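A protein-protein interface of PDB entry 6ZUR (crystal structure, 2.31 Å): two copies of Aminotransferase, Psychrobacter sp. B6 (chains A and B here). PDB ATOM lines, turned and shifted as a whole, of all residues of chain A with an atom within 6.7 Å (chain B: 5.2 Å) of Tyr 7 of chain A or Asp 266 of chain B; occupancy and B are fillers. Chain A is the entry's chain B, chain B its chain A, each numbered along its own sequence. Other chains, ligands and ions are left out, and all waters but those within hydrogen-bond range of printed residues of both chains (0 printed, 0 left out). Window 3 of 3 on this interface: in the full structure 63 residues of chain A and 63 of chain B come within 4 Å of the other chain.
The side-chain amide nitrogen (NE2) of Gln 274 of chain B sits close to the backbone NH (N) of Tyr 8 of chain A. The side-chain carboxylate (OD1) of Asp 266 of chain B lies within hydrogen-bond range of the side-chain hydroxyl (OH) of Tyr 7 of chain A, 2.7 Å away. The side-chain amide nitrogen (NE2) of Gln 274 of chain B sits at hydrogen-bond distance from the backbone carbonyl oxygen (O) of Asp 6 of chain A, 3.1 Å away. The guanidinium group of Arg 270 of chain B is in hydrogen-bond range of the backbone carbonyl oxygen of Ile 5 of chain A (2.5 Å). NH2 of Arg 270 of chain B lies within hydrogen-bond range of OH of Tyr 7 of chain A (3.1 Å). The backbone NH (N) of Phe 2 of chain A lies within hydrogen-bond range of the side-chain carboxylate (OE1) of Glu 267 of chain B.
Of the 8 printed residues of chain A, 6 touch a printed residue of chain B. Among the printed residues, 12 pairs touch across the chains.
Of the printed residues of chain B, Ile 5 of chain A touches Arg 270 and Gln 274. Of the printed residues of chain B, Asp 6 of chain A touches Arg 270 and Gln 274. Printed residues of chain B within 4 Å of Tyr 8 of chain A: Gln 274. Gly 10 of chain A touches none of the printed residues of chain B. Asp 266 of chain B touches just one residue of chain A: Tyr 7 (2.7 Å). Printed residues of chain A within 4 Å of Glu 267 of chain B: Phe 2 and Glu 3. Printed residues of chain A within 4 Å of Gln 274 of chain B: Ile 5 (3.4 Å), Asp 6 (3.1 Å), Tyr 7 (3.6 Å) and Tyr 8 (3.4 Å). The nearest residue of chain A that does not touch Asp 266 of chain B is Glu 3 of chain A (6.4 Å). The nearest printed residue of chain A that does not touch Glu 267 of chain B is Ile 5 of chain A (5.9 Å).
The side-chain hydroxyl of Thr 264 of chain B lies within hydrogen-bond range of the side-chain carboxylate of Glu 267 of chain B. OD2 of Asp 266 of chain B lies within salt-bridge range of NE of Arg 270 of chain B (3.1 Å).
CD of Arg 270 of chain B touches O of Phe 2 of chain A, at 3.8 Å. OE1 of Glu 3 of chain A touches OE1 of Glu 267 of chain B, 3.7 Å away. Glu 3 of chain A touches Arg 270 of chain B. CG2 of Ile 5 of chain A touches CG of Gln 274 of chain B (3.4 Å). O of Asp 6 of chain A touches O of Arg 270 of chain B, 3.9 Å away. Tyr 7 of chain A touches Gln 274 of chain B.
No position is printed for both chains.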
ATOM      1  N   PHE A   2      14.165 -15.980 -16.038  1.00  0.00           N
ATOM      2  CA  PHE A   2      14.123 -14.683 -15.393  1.00  0.00           C
ATOM      3  C   PHE A   2      13.060 -14.606 -14.292  1.00  0.00           C
ATOM      4  O   PHE A   2      12.633 -13.506 -13.931  1.00  0.00           O
ATOM      5  CB  PHE A   2      13.871 -13.603 -16.451  1.00  0.00           C
ATOM      6  CG  PHE A   2      14.882 -13.597 -17.559  1.00  0.00           C
ATOM      7  CD1 PHE A   2      16.215 -13.289 -17.284  1.00  0.00           C
ATOM      8  CD2 PHE A   2      14.512 -13.884 -18.878  1.00  0.00           C
ATOM      9  CE1 PHE A   2      17.174 -13.284 -18.301  1.00  0.00           C
ATOM     10  CE2 PHE A   2      15.462 -13.880 -19.898  1.00  0.00           C
ATOM     11  CZ  PHE A   2      16.793 -13.568 -19.603  1.00  0.00           C
ATOM     12  N   GLU A   3      12.657 -15.743 -13.723  1.00  0.00           N
ATOM     13  CA  GLU A   3      11.781 -15.716 -12.554  1.00  0.00           C
ATOM     14  C   GLU A   3      12.459 -15.053 -11.333  1.00  0.00           C
ATOM     15  O   GLU A   3      11.772 -14.550 -10.433  1.00  0.00           O
ATOM     16  CB  GLU A   3      11.257 -17.130 -12.188  1.00  0.00           C
ATOM     17  CG  GLU A   3      12.302 -18.160 -11.730  1.00  0.00           C
ATOM     18  CD  GLU A   3      13.077 -18.802 -12.875  1.00  0.00           C
ATOM     19  OE1 GLU A   3      13.034 -18.276 -14.006  1.00  0.00           O
ATOM     20  OE2 GLU A   3      13.720 -19.844 -12.648  1.00  0.00           O
ATOM     21  N   ILE A   5      13.964 -12.346 -11.512  1.00  0.00           N
ATOM     22  CA  ILE A   5      13.744 -10.924 -11.775  1.00  0.00           C
ATOM     23  C   ILE A   5      12.466 -10.432 -11.108  1.00  0.00           C
ATOM     24  O   ILE A   5      11.363 -10.895 -11.363  1.00  0.00           O
ATOM     25  CB  ILE A   5      13.701 -10.552 -13.281  1.00  0.00           C
ATOM     26  CG1 ILE A   5      14.884 -11.154 -14.053  1.00  0.00           C
ATOM     27  CG2 ILE A   5      13.733  -9.048 -13.457  1.00  0.00           C
ATOM     28  CD1 ILE A   5      16.260 -10.881 -13.498  1.00  0.00           C
ATOM     29  N   ASP A   6      12.671  -9.458 -10.253  1.00  0.00           N
ATOM     30  CA  ASP A   6      11.634  -8.741  -9.587  1.00  0.00           C
ATOM     31  C   ASP A   6      10.972  -7.791 -10.605  1.00  0.00           C
ATOM     32  O   ASP A   6      11.634  -7.346 -11.555  1.00  0.00           O
ATOM     33  CB  ASP A   6      12.329  -7.961  -8.474  1.00  0.00           C
ATOM     34  CG  ASP A   6      11.408  -7.479  -7.428  1.00  0.00           C
ATOM     35  OD1 ASP A   6      10.186  -7.752  -7.525  1.00  0.00           O
ATOM     36  OD2 ASP A   6      11.908  -6.823  -6.498  1.00  0.00           O
ATOM     37  N   TYR A   7       9.680  -7.507 -10.428  1.00  0.00           N
ATOM     38  CA  TYR A   7       8.979  -6.528 -11.285  1.00  0.00           C
ATOM     39  C   TYR A   7       9.496  -5.190 -10.818  1.00  0.00           C
ATOM     40  O   TYR A   7       9.706  -5.003  -9.625  1.00  0.00           O
ATOM     41  CB  TYR A   7       7.427  -6.542 -11.107  1.00  0.00           C
ATOM     42  CG  TYR A   7       6.776  -7.852 -11.470  1.00  0.00           C
ATOM     43  CD1 TYR A   7       6.390  -8.122 -12.780  1.00  0.00           C
ATOM     44  CD2 TYR A   7       6.576  -8.846 -10.493  1.00  0.00           C
ATOM     45  CE1 TYR A   7       5.815  -9.342 -13.119  1.00  0.00           C
ATOM     46  CE2 TYR A   7       6.001 -10.066 -10.810  1.00  0.00           C
ATOM     47  CZ  TYR A   7       5.607 -10.313 -12.121  1.00  0.00           C
ATOM     48  OH  TYR A   7       5.023 -11.531 -12.411  1.00  0.00           O
ATOM     49  N   TYR A   8       9.686  -4.268 -11.743  1.00  0.00           N
ATOM     50  CA  TYR A   8      10.008  -2.891 -11.378  1.00  0.00           C
ATOM     51  C   TYR A   8       8.725  -2.113 -11.218  1.00  0.00           C
ATOM     52  O   TYR A   8       7.917  -2.069 -12.126  1.00  0.00           O
ATOM     53  CB  TYR A   8      10.887  -2.265 -12.435  1.00  0.00           C
ATOM     54  CG  TYR A   8      11.146  -0.795 -12.232  1.00  0.00           C
ATOM     55  CD1 TYR A   8      11.713  -0.319 -11.054  1.00  0.00           C
ATOM     56  CD2 TYR A   8      10.834   0.123 -13.245  1.00  0.00           C
ATOM     57  CE1 TYR A   8      11.937   1.032 -10.886  1.00  0.00           C
ATOM     58  CE2 TYR A   8      11.059   1.469 -13.097  1.00  0.00           C
ATOM     59  CZ  TYR A   8      11.617   1.922 -11.939  1.00  0.00           C
ATOM     60  OH  TYR A   8      11.814   3.269 -11.856  1.00  0.00           O
ATOM     61  N   ALA A   9       8.567  -1.505 -10.049  1.00  0.00           N
ATOM     62  CA  ALA A   9       7.380  -0.744  -9.689  1.00  0.00           C
ATOM     63  C   ALA A   9       7.029   0.396 -10.660  1.00  0.00           C
ATOM     64  O   ALA A   9       5.861   0.733 -10.791  1.00  0.00           O
ATOM     65  CB  ALA A   9       7.551  -0.184  -8.280  1.00  0.00           C
ATOM     66  N   GLY A  10       8.037   0.991 -11.304  1.00  0.00           N
ATOM     67  CA  GLY A  10       7.843   2.080 -12.269  1.00  0.00           C
ATOM     68  C   GLY A  10       8.168   3.399 -11.590  1.00  0.00           C
ATOM     69  O   GLY A  10       8.059   3.514 -10.358  1.00  0.00           O
ATOM     70  N   THR B 264       8.805 -16.299 -21.613  1.00  0.00           N
ATOM     71  CA  THR B 264       7.372 -16.022 -21.469  1.00  0.00           C
ATOM     72  C   THR B 264       7.095 -14.545 -21.384  1.00  0.00           C
ATOM     73  O   THR B 264       7.931 -13.774 -20.946  1.00  0.00           O
ATOM     74  CB  THR B 264       6.803 -16.648 -20.180  1.00  0.00           C
ATOM     75  OG1 THR B 264       7.406 -16.030 -19.042  1.00  0.00           O
ATOM     76  CG2 THR B 264       7.070 -18.092 -20.110  1.00  0.00           C
ATOM     77  N   VAL B 265       5.875 -14.168 -21.722  1.00  0.00           N
ATOM     78  CA  VAL B 265       5.459 -12.759 -21.742  1.00  0.00           C
ATOM     79  C   VAL B 265       5.643 -12.099 -20.409  1.00  0.00           C
ATOM     80  O   VAL B 265       5.981 -10.946 -20.354  1.00  0.00           O
ATOM     81  CB  VAL B 265       4.002 -12.626 -22.152  1.00  0.00           C
ATOM     82  CG1 VAL B 265       3.504 -11.189 -22.027  1.00  0.00           C
ATOM     83  CG2 VAL B 265       3.876 -13.063 -23.592  1.00  0.00           C
ATOM     84  N   ASP B 266       5.428 -12.863 -19.349  1.00  0.00           N
ATOM     85  CA  ASP B 266       5.502 -12.379 -18.009  1.00  0.00           C
ATOM     86  C   ASP B 266       6.939 -12.021 -17.640  1.00  0.00           C
ATOM     87  O   ASP B 266       7.181 -10.960 -17.051  1.00  0.00           O
ATOM     88  CB  ASP B 266       4.946 -13.445 -17.052  1.00  0.00           C
ATOM     89  CG  ASP B 266       5.326 -13.172 -15.617  1.00  0.00           C
ATOM     90  OD1 ASP B 266       4.783 -12.203 -15.034  1.00  0.00           O
ATOM     91  OD2 ASP B 266       6.194 -13.905 -15.088  1.00  0.00           O
ATOM     92  N   GLU B 267       7.868 -12.920 -17.980  1.00  0.00           N
ATOM     93  CA  GLU B 267       9.315 -12.671 -17.862  1.00  0.00           C
ATOM     94  C   GLU B 267       9.726 -11.474 -18.698  1.00  0.00           C
ATOM     95  O   GLU B 267      10.584 -10.719 -18.296  1.00  0.00           O
ATOM     96  CB  GLU B 267      10.156 -13.884 -18.281  1.00  0.00           C
ATOM     97  CG  GLU B 267      10.537 -14.825 -17.129  1.00  0.00           C
ATOM     98  CD  GLU B 267      10.816 -16.251 -17.596  1.00  0.00           C
ATOM     99  OE1 GLU B 267      11.863 -16.836 -17.219  1.00  0.00           O
ATOM    100  OE2 GLU B 267       9.987 -16.797 -18.353  1.00  0.00           O
ATOM    101  N   THR B 268       9.083 -11.300 -19.851  1.00  0.00           N
ATOM    102  CA  THR B 268       9.352 -10.150 -20.744  1.00  0.00           C
ATOM    103  C   THR B 268       9.065  -8.859 -19.997  1.00  0.00           C
ATOM    104  O   THR B 268       9.847  -7.924 -20.038  1.00  0.00           O
ATOM    105  CB  THR B 268       8.511 -10.253 -22.066  1.00  0.00           C
ATOM    106  OG1 THR B 268       8.903 -11.446 -22.739  1.00  0.00           O
ATOM    107  CG2 THR B 268       8.691  -9.020 -23.019  1.00  0.00           C
ATOM    108  N   GLU B 269       7.943  -8.832 -19.301  1.00  0.00           N
ATOM    109  CA  GLU B 269       7.566  -7.672 -18.532  1.00  0.00           C
ATOM    110  C   GLU B 269       8.495  -7.465 -17.332  1.00  0.00           C
ATOM    111  O   GLU B 269       8.802  -6.353 -17.017  1.00  0.00           O
ATOM    112  CB  GLU B 269       6.120  -7.784 -18.057  1.00  0.00           C
ATOM    113  CG  GLU B 269       5.081  -7.650 -19.159  1.00  0.00           C
ATOM    114  CD  GLU B 269       3.661  -7.885 -18.644  1.00  0.00           C
ATOM    115  OE1 GLU B 269       3.446  -7.804 -17.408  1.00  0.00           O
ATOM    116  OE2 GLU B 269       2.759  -8.143 -19.475  1.00  0.00           O
ATOM    117  N   ARG B 270       8.924  -8.517 -16.646  1.00  0.00           N
ATOM    118  CA  ARG B 270       9.877  -8.341 -15.497  1.00  0.00           C
ATOM    119  C   ARG B 270      11.190  -7.699 -15.988  1.00  0.00           C
ATOM    120  O   ARG B 270      11.697  -6.748 -15.431  1.00  0.00           O
ATOM    121  CB  ARG B 270      10.189  -9.662 -14.847  1.00  0.00           C
ATOM    122  CG  ARG B 270       9.004 -10.335 -14.172  1.00  0.00           C
ATOM    123  CD  ARG B 270       9.250 -11.824 -14.023  1.00  0.00           C
ATOM    124  NE  ARG B 270       8.231 -12.549 -13.258  1.00  0.00           N
ATOM    125  CZ  ARG B 270       8.257 -12.719 -11.931  1.00  0.00           C
ATOM    126  NH1 ARG B 270       9.246 -12.189 -11.202  1.00  0.00           N
ATOM    127  NH2 ARG B 270       7.292 -13.405 -11.331  1.00  0.00           N
ATOM    128  N   GLN B 274      12.894  -3.936 -15.521  1.00  0.00           N
ATOM    129  CA  GLN B 274      14.204  -3.780 -14.886  1.00  0.00           C
ATOM    130  C   GLN B 274      15.216  -3.090 -15.807  1.00  0.00           C
ATOM    131  O   GLN B 274      16.108  -2.402 -15.319  1.00  0.00           O
ATOM    132  CB  GLN B 274      14.709  -5.113 -14.439  1.00  0.00           C
ATOM    133  CG  GLN B 274      13.972  -5.636 -13.250  1.00  0.00           C
ATOM    134  CD  GLN B 274      14.083  -4.745 -12.034  1.00  0.00           C
ATOM    135  OE1 GLN B 274      15.094  -4.146 -11.798  1.00  0.00           O
ATOM    136  NE2 GLN B 274      13.017  -4.632 -11.298  1.00  0.00           N
